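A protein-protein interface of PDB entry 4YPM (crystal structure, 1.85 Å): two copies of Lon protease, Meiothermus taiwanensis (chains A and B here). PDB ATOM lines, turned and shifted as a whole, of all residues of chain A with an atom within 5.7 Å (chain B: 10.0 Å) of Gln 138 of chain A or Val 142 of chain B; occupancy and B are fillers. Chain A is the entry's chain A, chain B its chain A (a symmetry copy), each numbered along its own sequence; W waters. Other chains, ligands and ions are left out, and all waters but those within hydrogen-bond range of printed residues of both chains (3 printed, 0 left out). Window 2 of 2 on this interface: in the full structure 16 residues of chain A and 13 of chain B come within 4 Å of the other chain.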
ATOM      1  N   LEU A 135      -1.400 -19.988  12.231  1.00  0.00           N
ATOM      2  CA  LEU A 135      -0.371 -19.491  13.136  1.00  0.00           C
ATOM      3  C   LEU A 135      -0.928 -18.286  13.891  1.00  0.00           C
ATOM      4  O   LEU A 135      -1.047 -17.181  13.316  1.00  0.00           O
ATOM      5  CB  LEU A 135       0.880 -19.080  12.332  1.00  0.00           C
ATOM      6  CG  LEU A 135       1.494 -20.134  11.410  1.00  0.00           C
ATOM      7  CD1 LEU A 135       2.534 -19.558  10.472  1.00  0.00           C
ATOM      8  CD2 LEU A 135       2.076 -21.262  12.237  1.00  0.00           C
ATOM      9  N   THR A 136      -1.258 -18.468  15.161  1.00  0.00           N
ATOM     10  CA  THR A 136      -1.983 -17.459  15.903  1.00  0.00           C
ATOM     11  C   THR A 136      -1.307 -17.128  17.231  1.00  0.00           C
ATOM     12  O   THR A 136      -0.383 -17.829  17.675  1.00  0.00           O
ATOM     13  CB  THR A 136      -3.463 -17.853  16.136  1.00  0.00           C
ATOM     14  OG1 THR A 136      -3.542 -19.068  16.906  1.00  0.00           O
ATOM     15  CG2 THR A 136      -4.203 -18.033  14.807  1.00  0.00           C
ATOM     16  N   GLY A 137      -1.797 -16.068  17.868  1.00  0.00           N
ATOM     17  CA  GLY A 137      -1.149 -15.482  19.048  1.00  0.00           C
ATOM     18  C   GLY A 137      -0.341 -14.228  18.710  1.00  0.00           C
ATOM     19  O   GLY A 137       0.607 -13.884  19.422  1.00  0.00           O
ATOM     20  N   GLN A 138      -0.759 -13.535  17.646  1.00  0.00           N
ATOM     21  CA  GLN A 138      -0.149 -12.255  17.215  1.00  0.00           C
ATOM     22  C   GLN A 138       1.340 -12.406  16.918  1.00  0.00           C
ATOM     23  O   GLN A 138       2.191 -11.634  17.403  1.00  0.00           O
ATOM     24  CB  GLN A 138      -0.426 -11.147  18.246  1.00  0.00           C
ATOM     25  CG  GLN A 138      -1.925 -10.807  18.371  1.00  0.00           C
ATOM     26  CD  GLN A 138      -2.485 -10.246  17.094  1.00  0.00           C
ATOM     27  OE1 GLN A 138      -3.115 -10.954  16.299  1.00  0.00           O
ATOM     28  NE2 GLN A 138      -2.244  -8.983  16.863  1.00  0.00           N
ATOM     29  N   LEU A 139       1.640 -13.394  16.080  1.00  0.00           N
ATOM     30  CA  LEU A 139       2.998 -13.738  15.733  1.00  0.00           C
ATOM     31  C   LEU A 139       3.464 -12.862  14.578  1.00  0.00           C
ATOM     32  O   LEU A 139       2.775 -12.755  13.567  1.00  0.00           O
ATOM     33  CB  LEU A 139       3.094 -15.196  15.311  1.00  0.00           C
ATOM     34  CG  LEU A 139       2.383 -16.200  16.233  1.00  0.00           C
ATOM     35  CD1 LEU A 139       2.662 -17.601  15.734  1.00  0.00           C
ATOM     36  CD2 LEU A 139       2.790 -16.049  17.688  1.00  0.00           C
ATOM     37  N   GLY A 140       4.663 -12.316  14.701  1.00  0.00           N
ATOM     38  CA  GLY A 140       5.292 -11.564  13.614  1.00  0.00           C
ATOM     39  C   GLY A 140       5.779 -12.431  12.467  1.00  0.00           C
ATOM     40  O   GLY A 140       5.871 -13.666  12.560  1.00  0.00           O
ATOM     41  N   VAL A 177       0.348 -19.367  20.294  1.00  0.00           N
ATOM     42  CA  VAL A 177       1.179 -18.969  21.409  1.00  0.00           C
ATOM     43  C   VAL A 177       0.433 -17.962  22.262  1.00  0.00           C
ATOM     44  O   VAL A 177       0.373 -16.772  21.936  1.00  0.00           O
ATOM     45  CB  VAL A 177       2.559 -18.428  20.981  1.00  0.00           C
ATOM     46  CG1 VAL A 177       3.462 -18.349  22.186  1.00  0.00           C
ATOM     47  CG2 VAL A 177       3.175 -19.319  19.922  1.00  0.00           C
ATOM     48  N   GLY A 180      -3.355 -14.356  23.940  1.00  0.00           N
ATOM     49  CA  GLY A 180      -3.852 -13.976  22.621  1.00  0.00           C
ATOM     50  C   GLY A 180      -3.509 -12.571  22.154  1.00  0.00           C
ATOM     51  O   GLY A 180      -3.299 -12.349  20.954  1.00  0.00           O
ATOM     52  N   ALA A 181      -3.464 -11.618  23.076  1.00  0.00           N
ATOM     53  CA  ALA A 181      -3.326 -10.203  22.709  1.00  0.00           C
ATOM     54  C   ALA A 181      -1.888  -9.701  22.527  1.00  0.00           C
ATOM     55  O   ALA A 181      -1.667  -8.702  21.842  1.00  0.00           O
ATOM     56  CB  ALA A 181      -4.049  -9.343  23.723  1.00  0.00           C
ATOM     57  N   THR A 182      -0.924 -10.369  23.127  1.00  0.00           N
ATOM     58  CA  THR A 182       0.460  -9.872  23.204  1.00  0.00           C
ATOM     59  C   THR A 182       1.227 -10.190  21.920  1.00  0.00           C
ATOM     60  O   THR A 182       1.359 -11.345  21.542  1.00  0.00           O
ATOM     61  CB  THR A 182       1.197 -10.494  24.394  1.00  0.00           C
ATOM     62  OG1 THR A 182       0.458 -10.197  25.584  1.00  0.00           O
ATOM     63  CG2 THR A 182       2.633  -9.949  24.535  1.00  0.00           C
ATOM     64  N   PRO A 183       1.746  -9.157  21.246  1.00  0.00           N
ATOM     65  CA  PRO A 183       2.570  -9.458  20.087  1.00  0.00           C
ATOM     66  C   PRO A 183       3.828 -10.211  20.439  1.00  0.00           C
ATOM     67  O   PRO A 183       4.428  -9.971  21.478  1.00  0.00           O
ATOM     68  CB  PRO A 183       2.924  -8.071  19.532  1.00  0.00           C
ATOM     69  CG  PRO A 183       1.860  -7.186  20.054  1.00  0.00           C
ATOM     70  CD  PRO A 183       1.548  -7.707  21.417  1.00  0.00           C
ATOM     71  N   LYS A 184       4.203 -11.140  19.566  1.00  0.00           N
ATOM     72  CA  LYS A 184       5.393 -11.958  19.721  1.00  0.00           C
ATOM     73  C   LYS A 184       6.121 -12.026  18.386  1.00  0.00           C
ATOM     74  O   LYS A 184       5.505 -12.008  17.327  1.00  0.00           O
ATOM     75  CB  LYS A 184       5.030 -13.369  20.165  1.00  0.00           C
ATOM     76  CG  LYS A 184       4.055 -13.380  21.322  1.00  0.00           C
ATOM     77  CD  LYS A 184       3.487 -14.734  21.614  1.00  0.00           C
ATOM     78  CE  LYS A 184       2.461 -14.568  22.715  1.00  0.00           C
ATOM     79  NZ  LYS A 184       1.160 -14.043  22.224  1.00  0.00           N
ATOM     80  N   ASP A 185       7.437 -12.100  18.428  1.00  0.00           N
ATOM     81  CA  ASP A 185       8.190 -12.228  17.183  1.00  0.00           C
ATOM     82  C   ASP A 185       9.577 -12.797  17.439  1.00  0.00           C
ATOM     83  O   ASP A 185       9.999 -12.958  18.579  1.00  0.00           O
ATOM     84  CB  ASP A 185       8.291 -10.869  16.469  1.00  0.00           C
ATOM     85  CG  ASP A 185       8.498 -10.998  14.975  1.00  0.00           C
ATOM     86  OD1 ASP A 185       8.532 -12.132  14.420  1.00  0.00           O
ATOM     87  OD2 ASP A 185       8.628  -9.945  14.317  1.00  0.00           O
ATOM     88  N   LEU B 135     -16.344 -14.678   9.902  1.00  0.00           N
ATOM     89  CA  LEU B 135     -16.276 -14.015  11.199  1.00  0.00           C
ATOM     90  C   LEU B 135     -16.680 -12.552  11.019  1.00  0.00           C
ATOM     91  O   LEU B 135     -15.888 -11.740  10.490  1.00  0.00           O
ATOM     92  CB  LEU B 135     -14.842 -14.103  11.760  1.00  0.00           C
ATOM     93  CG  LEU B 135     -14.224 -15.497  11.881  1.00  0.00           C
ATOM     94  CD1 LEU B 135     -12.740 -15.457  12.175  1.00  0.00           C
ATOM     95  CD2 LEU B 135     -14.965 -16.295  12.934  1.00  0.00           C
ATOM     96  N   GLN B 138     -17.580  -6.802  12.701  1.00  0.00           N
ATOM     97  CA  GLN B 138     -16.437  -5.870  12.838  1.00  0.00           C
ATOM     98  C   GLN B 138     -15.468  -6.314  13.933  1.00  0.00           C
ATOM     99  O   GLN B 138     -15.077  -5.533  14.823  1.00  0.00           O
ATOM    100  CB  GLN B 138     -16.933  -4.430  13.052  1.00  0.00           C
ATOM    101  CG  GLN B 138     -17.703  -3.877  11.836  1.00  0.00           C
ATOM    102  CD  GLN B 138     -16.832  -3.770  10.616  1.00  0.00           C
ATOM    103  OE1 GLN B 138     -16.847  -4.637   9.734  1.00  0.00           O
ATOM    104  NE2 GLN B 138     -16.044  -2.729  10.559  1.00  0.00           N
ATOM    105  N   LEU B 139     -15.059  -7.574  13.831  1.00  0.00           N
ATOM    106  CA  LEU B 139     -14.199  -8.197  14.808  1.00  0.00           C
ATOM    107  C   LEU B 139     -12.746  -7.889  14.475  1.00  0.00           C
ATOM    108  O   LEU B 139     -12.317  -8.082  13.341  1.00  0.00           O
ATOM    109  CB  LEU B 139     -14.391  -9.705  14.813  1.00  0.00           C
ATOM    110  CG  LEU B 139     -15.851 -10.187  14.828  1.00  0.00           C
ATOM    111  CD1 LEU B 139     -15.864 -11.696  14.938  1.00  0.00           C
ATOM    112  CD2 LEU B 139     -16.665  -9.553  15.943  1.00  0.00           C
ATOM    113  N   GLY B 140     -11.983  -7.497  15.483  1.00  0.00           N
ATOM    114  CA  GLY B 140     -10.539  -7.298  15.336  1.00  0.00           C
ATOM    115  C   GLY B 140      -9.750  -8.589  15.209  1.00  0.00           C
ATOM    116  O   GLY B 140     -10.244  -9.699  15.466  1.00  0.00           O
ATOM    117  N   GLU B 141      -8.483  -8.448  14.837  1.00  0.00           N
ATOM    118  CA  GLU B 141      -7.664  -9.616  14.542  1.00  0.00           C
ATOM    119  C   GLU B 141      -7.480 -10.537  15.744  1.00  0.00           C
ATOM    120  O   GLU B 141      -7.592 -11.742  15.597  1.00  0.00           O
ATOM    121  CB  GLU B 141      -6.305  -9.208  13.936  1.00  0.00           C
ATOM    122  CG  GLU B 141      -6.465  -8.464  12.604  1.00  0.00           C
ATOM    123  CD  GLU B 141      -7.233  -9.266  11.538  1.00  0.00           C
ATOM    124  OE1 GLU B 141      -8.324  -8.834  11.092  1.00  0.00           O
ATOM    125  OE2 GLU B 141      -6.765 -10.350  11.138  1.00  0.00           O
ATOM    126  N   VAL B 142      -7.229  -9.987  16.929  1.00  0.00           N
ATOM    127  CA  VAL B 142      -7.121 -10.806  18.136  1.00  0.00           C
ATOM    128  C   VAL B 142      -8.408 -11.618  18.393  1.00  0.00           C
ATOM    129  O   VAL B 142      -8.365 -12.805  18.754  1.00  0.00           O
ATOM    130  CB  VAL B 142      -6.777  -9.926  19.354  1.00  0.00           C
ATOM    131  CG1 VAL B 142      -6.961 -10.694  20.659  1.00  0.00           C
ATOM    132  CG2 VAL B 142      -5.329  -9.417  19.237  1.00  0.00           C
ATOM    133  N   MET B 143      -9.559 -10.972  18.246  1.00  0.00           N
ATOM    134  CA  MET B 143     -10.813 -11.693  18.452  1.00  0.00           C
ATOM    135  C   MET B 143     -11.029 -12.772  17.387  1.00  0.00           C
ATOM    136  O   MET B 143     -11.523 -13.873  17.678  1.00  0.00           O
ATOM    137  CB  MET B 143     -11.974 -10.733  18.519  1.00  0.00           C
ATOM    138  CG  MET B 143     -13.297 -11.370  18.887  1.00  0.00           C
ATOM    139  SD  MET B 143     -14.481 -10.055  19.221  1.00  0.00           S
ATOM    140  CE  MET B 143     -15.985 -11.021  19.440  1.00  0.00           C
ATOM    141  N   LYS B 144     -10.629 -12.486  16.161  1.00  0.00           N
ATOM    142  CA  LYS B 144     -10.720 -13.499  15.116  1.00  0.00           C
ATOM    143  C   LYS B 144      -9.826 -14.704  15.395  1.00  0.00           C
ATOM    144  O   LYS B 144     -10.237 -15.858  15.157  1.00  0.00           O
ATOM    145  CB  LYS B 144     -10.449 -12.917  13.749  1.00  0.00           C
ATOM    146  CG  LYS B 144     -11.572 -12.024  13.277  1.00  0.00           C
ATOM    147  CD  LYS B 144     -11.302 -11.612  11.843  1.00  0.00           C
ATOM    148  CE  LYS B 144     -12.389 -10.750  11.246  1.00  0.00           C
ATOM    149  NZ  LYS B 144     -11.814 -10.142   9.998  1.00  0.00           N
ATOM    150  N   GLU B 145      -8.615 -14.462  15.891  1.00  0.00           N
ATOM    151  CA  GLU B 145      -7.699 -15.561  16.246  1.00  0.00           C
ATOM    152  C   GLU B 145      -8.269 -16.397  17.403  1.00  0.00           C
ATOM    153  O   GLU B 145      -8.100 -17.612  17.443  1.00  0.00           O
ATOM    154  CB  GLU B 145      -6.293 -15.036  16.584  1.00  0.00           C
ATOM    155  CG  GLU B 145      -5.552 -14.487  15.367  1.00  0.00           C
ATOM    156  CD  GLU B 145      -4.071 -14.209  15.586  1.00  0.00           C
ATOM    157  OE1 GLU B 145      -3.570 -14.142  16.736  1.00  0.00           O
ATOM    158  OE2 GLU B 145      -3.394 -14.049  14.553  1.00  0.00           O
ATOM    159  N   SER B 146      -8.961 -15.733  18.319  1.00  0.00           N
ATOM    160  CA  SER B 146      -9.629 -16.382  19.427  1.00  0.00           C
ATOM    161  C   SER B 146     -10.686 -17.360  18.911  1.00  0.00           C
ATOM    162  O   SER B 146     -10.792 -18.489  19.405  1.00  0.00           O
ATOM    163  CB  SER B 146     -10.249 -15.322  20.319  1.00  0.00           C
ATOM    164  OG  SER B 146     -11.075 -15.872  21.286  1.00  0.00           O
ATOM    165  N   ALA B 147     -11.467 -16.928  17.923  1.00  0.00           N
ATOM    166  CA  ALA B 147     -12.454 -17.825  17.292  1.00  0.00           C
ATOM    167  C   ALA B 147     -11.783 -19.032  16.641  1.00  0.00           C
ATOM    168  O   ALA B 147     -12.275 -20.170  16.740  1.00  0.00           O
ATOM    169  CB  ALA B 147     -13.280 -17.084  16.275  1.00  0.00           C
ATOM    170  N   GLN B 148     -10.661 -18.791  15.975  1.00  0.00           N
ATOM    171  CA  GLN B 148      -9.917 -19.865  15.343  1.00  0.00           C
ATOM    172  C   GLN B 148      -9.394 -20.868  16.381  1.00  0.00           C
ATOM    173  O   GLN B 148      -9.466 -22.069  16.162  1.00  0.00           O
ATOM    174  CB  GLN B 148      -8.767 -19.322  14.513  1.00  0.00           C
ATOM    175  CG  GLN B 148      -9.187 -18.510  13.300  1.00  0.00           C
ATOM    176  CD  GLN B 148      -7.985 -18.103  12.481  1.00  0.00           C
ATOM    177  OE1 GLN B 148      -7.648 -18.754  11.481  1.00  0.00           O
ATOM    178  NE2 GLN B 148      -7.293 -17.112  12.928  1.00  0.00           N
ATOM    179  N   ALA B 149      -8.896 -20.367  17.518  1.00  0.00           N
ATOM    180  CA  ALA B 149      -8.394 -21.251  18.570  1.00  0.00           C
ATOM    181  C   ALA B 149      -9.526 -22.104  19.154  1.00  0.00           C
ATOM    182  O   ALA B 149      -9.364 -23.314  19.346  1.00  0.00           O
ATOM    183  CB  ALA B 149      -7.734 -20.456  19.668  1.00  0.00           C
ATOM    184  N   ALA B 150     -10.671 -21.477  19.399  1.00  0.00           N
ATOM    185  CA  ALA B 150     -11.860 -22.202  19.878  1.00  0.00           C
ATOM    186  C   ALA B 150     -12.279 -23.305  18.898  1.00  0.00           C
ATOM    187  O   ALA B 150     -12.540 -24.446  19.304  1.00  0.00           O
ATOM    188  CB  ALA B 150     -13.008 -21.240  20.134  1.00  0.00           C
ATOM    189  N   LYS B 184     -15.427  -4.526  17.622  1.00  0.00           N
ATOM    190  CA  LYS B 184     -15.215  -5.373  18.784  1.00  0.00           C
ATOM    191  C   LYS B 184     -13.848  -6.032  18.671  1.00  0.00           C
ATOM    192  O   LYS B 184     -13.379  -6.336  17.580  1.00  0.00           O
ATOM    193  CB  LYS B 184     -16.285  -6.453  18.873  1.00  0.00           C
ATOM    194  CG  LYS B 184     -17.683  -5.900  18.692  1.00  0.00           C
ATOM    195  CD  LYS B 184     -18.728  -6.959  18.520  1.00  0.00           C
ATOM    196  CE  LYS B 184     -20.043  -6.259  18.248  1.00  0.00           C
ATOM    197  NZ  LYS B 184     -20.173  -5.793  16.843  1.00  0.00           N
ATOM    198  N   ASP B 185     -13.199  -6.255  19.797  1.00  0.00           N
ATOM    199  CA  ASP B 185     -11.909  -6.940  19.760  1.00  0.00           C
ATOM    200  C   ASP B 185     -11.572  -7.545  21.114  1.00  0.00           C
ATOM    201  O   ASP B 185     -12.262  -7.318  22.102  1.00  0.00           O
ATOM    202  CB  ASP B 185     -10.796  -5.975  19.313  1.00  0.00           C
ATOM    203  CG  ASP B 185      -9.615  -6.683  18.685  1.00  0.00           C
ATOM    204  OD1 ASP B 185      -9.616  -7.936  18.531  1.00  0.00           O
ATOM    205  OD2 ASP B 185      -8.647  -5.982  18.324  1.00  0.00           O
ATOM    206  N   GLY B 186     -10.534  -8.372  21.119  1.00  0.00           N
ATOM    207  CA  GLY B 186      -9.983  -8.941  22.342  1.00  0.00           C
ATOM    208  C   GLY B 186     -10.157 -10.445  22.445  1.00  0.00           C
ATOM    209  O   GLY B 186     -10.932 -11.033  21.690  1.00  0.00           O
ATOM    210  N   PRO B 187      -9.424 -11.085  23.366  1.00  0.00           N
ATOM    211  CA  PRO B 187      -9.408 -12.542  23.461  1.00  0.00           C
ATOM    212  C   PRO B 187     -10.403 -13.123  24.464  1.00  0.00           C
ATOM    213  O   PRO B 187     -10.475 -14.342  24.608  1.00  0.00           O
ATOM    214  CB  PRO B 187      -7.990 -12.815  23.952  1.00  0.00           C
ATOM    215  CG  PRO B 187      -7.704 -11.646  24.852  1.00  0.00           C
ATOM    216  CD  PRO B 187      -8.366 -10.476  24.201  1.00  0.00           C
ATOM    217  N   SER B 188     -11.143 -12.272  25.165  1.00  0.00           N
ATOM    218  CA  SER B 188     -11.917 -12.713  26.333  1.00  0.00           C
ATOM    219  C   SER B 188     -13.258 -13.395  26.010  1.00  0.00           C
ATOM    220  O   SER B 188     -13.993 -13.775  26.921  1.00  0.00           O
ATOM    221  CB  SER B 188     -12.165 -11.545  27.275  1.00  0.00           C
ATOM    222  OG  SER B 188     -13.126 -10.678  26.722  1.00  0.00           O
ATOM    223  N   ALA B 189     -13.603 -13.486  24.733  1.00  0.00           N
ATOM    224  CA  ALA B 189     -14.781 -14.248  24.317  1.00  0.00           C
ATOM    225  C   ALA B 189     -14.410 -15.633  23.772  1.00  0.00           C
ATOM    226  O   ALA B 189     -15.222 -16.283  23.099  1.00  0.00           O
ATOM    227  CB  ALA B 189     -15.571 -13.458  23.300  1.00  0.00           C
ATOM    228  N   GLY B 190     -13.197 -16.115  24.082  1.00  0.00           N
ATOM    229  CA  GLY B 190     -12.772 -17.447  23.662  1.00  0.00           C
ATOM    230  C   GLY B 190     -13.702 -18.560  24.126  1.00  0.00           C
ATOM    231  O   GLY B 190     -14.133 -19.397  23.315  1.00  0.00           O
ATOM    232  N   MET B 193     -17.203 -18.066  22.403  1.00  0.00           N
ATOM    233  CA  MET B 193     -17.233 -18.610  21.047  1.00  0.00           C
ATOM    234  C   MET B 193     -17.164 -20.125  21.023  1.00  0.00           C
ATOM    235  O   MET B 193     -17.861 -20.762  20.218  1.00  0.00           O
ATOM    236  CB  MET B 193     -16.137 -17.980  20.209  1.00  0.00           C
ATOM    237  CG  MET B 193     -16.575 -16.562  19.863  1.00  0.00           C
ATOM    238  SD  MET B 193     -15.548 -15.625  18.766  1.00  0.00           S
ATOM    239  CE  MET B 193     -14.084 -15.556  19.799  1.00  0.00           C
ATOM    240  N   GLU B 215     -10.532 -16.061  28.222  1.00  0.00           N
ATOM    241  CA  GLU B 215      -9.677 -16.400  27.111  1.00  0.00           C
ATOM    242  C   GLU B 215      -9.471 -17.928  27.091  1.00  0.00           C
ATOM    243  O   GLU B 215      -9.418 -18.594  28.147  1.00  0.00           O
ATOM    244  CB  GLU B 215      -8.354 -15.619  27.210  1.00  0.00           C
ATOM    245  CG  GLU B 215      -7.289 -16.057  26.222  1.00  0.00           C
ATOM    246  CD  GLU B 215      -6.019 -15.195  26.237  1.00  0.00           C
ATOM    247  OE1 GLU B 215      -5.957 -14.164  26.956  1.00  0.00           O
ATOM    248  OE2 GLU B 215      -5.076 -15.586  25.526  1.00  0.00           O
ATOM    249  N   VAL B 216      -9.407 -18.490  25.894  1.00  0.00           N
ATOM    250  CA  VAL B 216      -9.155 -19.924  25.744  1.00  0.00           C
ATOM    251  C   VAL B 216      -7.796 -20.144  25.077  1.00  0.00           C
ATOM    252  O   VAL B 216      -7.426 -19.431  24.148  1.00  0.00           O
ATOM    253  CB  VAL B 216     -10.317 -20.616  24.986  1.00  0.00           C
ATOM    254  CG1 VAL B 216     -10.271 -20.325  23.494  1.00  0.00           C
ATOM    255  CG2 VAL B 216     -10.321 -22.117  25.271  1.00  0.00           C
HETATM  256  O   HOH W   1      -4.197 -14.307  19.333  1.00  0.00           O
HETATM  257  O   HOH W   2      -4.464 -12.011  25.966  1.00  0.00           O
HETATM  258  O   HOH W   3      -0.732 -14.396  14.432  1.00  0.00           O
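Positions printed for both chains: 135, 138, 139, 140, 184 and 185. Of the 7 pairs that touch across the chains among the printed residues, none has its exchanged pair printed and touching as well.
Of the printed residues of chain B, Thr 136 of chain A touches Glu 145 and Gln 148. Gly 137 of chain A touches just one residue of chain B: Glu 145. Of the printed residues of chain B, Gln 138 of chain A touches Val 142 and Glu 145. Leu 139 of chain A touches none of the printed residues of chain B. Printed residues of chain B within 4 Å of Gly 180 of chain A: Val 142 and Glu 215. No residue of chain B comes within 4 Å of Ala 181 of chain A. No residue of chain B comes within 4 Å of Pro 183 of chain A. Printed residues of chain A within 4 Å of Val 142 of chain B: Gln 138 and Gly 180. Printed residues of chain A within 4 Å of Glu 145 of chain B: Thr 136, Gly 137 and Gln 138. Ala 149 of chain B touches none of the printed residues of chain A. Printed residues of chain A within 4 Å of Glu 215 of chain B: Gly 180. The nearest residue of chain A that does not touch Val 142 of chain B is Ala 181 of chain A (4.1 Å).
The backbone NH (N) of Val 177 of chain A is in hydrogen-bond range of the backbone carbonyl oxygen (O) of Thr 136 of chain A. The side-chain amino group (NZ) of Lys 184 of chain A is in hydrogen-bond range of the backbone carbonyl oxygen (O) of Gly 137 of chain A (2.9 Å). The backbone NH (N) of Lys 184 of chain A sits at hydrogen-bond distance from the backbone carbonyl oxygen (O) of Gln 138 of chain A.
CB of Thr 136 of chain A touches CD of Glu 145 of chain B (3.7 Å). Gln 148 of chain B touches Thr 136 of chain A (NE2 to CG2, 3.7 Å). CD of Gln 138 of chain A touches CG2 of Val 142 of chain B, at 3.7 Å. O of Gly 180 of chain A touches CG2 of Val 142 of chain B, at 3.96 Å.
Of the 24 printed residues of chain B, 4 touch a printed residue of chain A. Printed residues of chain B that touch a printed residue of chain A: Val 142, Glu 145, Gln 148 and Glu 215. Hydrophobic or aromatic side chains of chain B within 4 Å of the printed part of chain A: Val 142. Along chain B the printed residues that touch a printed residue of chain A span positions 142 to 215. Among the printed residues, 7 pairs touch across the chains. Among the printed residues, no Asp or Glu carboxylate lies within 4 Å of a Lys or Arg side-chain nitrogen of the other chain.
The side-chain carboxylate (OE1) of Glu 145 of chain B is in hydrogen-bond range of the backbone NH (N) of Gly 137 of chain A. N of Gln 138 of chain A sits at hydrogen-bond distance from OE1 of Glu 145 of chain B (3.0 Å). The side-chain carboxylate (OE2) of Glu 215 of chain B is in hydrogen-bond range of the backbone NH (N) of Gly 180 of chain A.
Water W1 lies within hydrogen-bond range of OE1 of Glu 145 of chain B (2.7 Å), O of Gly 180 of chain A (2.7 Å) and N of Gly 137 of chain A (3.3 Å). Water W3 lies within hydrogen-bond range of the side-chain carboxylate (OE2) of Glu 145 of chain B, the backbone carbonyl oxygen (O) of Leu 135 of chain A, the backbone NH (N) of Leu 139 of chain A and the backbone NH (N) of Gln 138 of chain A. Water W2 lies within hydrogen-bond range of the side-chain carboxylate of Glu 215 of chain B (2.8 Å), the backbone NH of Ala 181 of chain A (3.1 Å) and the backbone NH of Gly 180 of chain A (3.3 Å).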
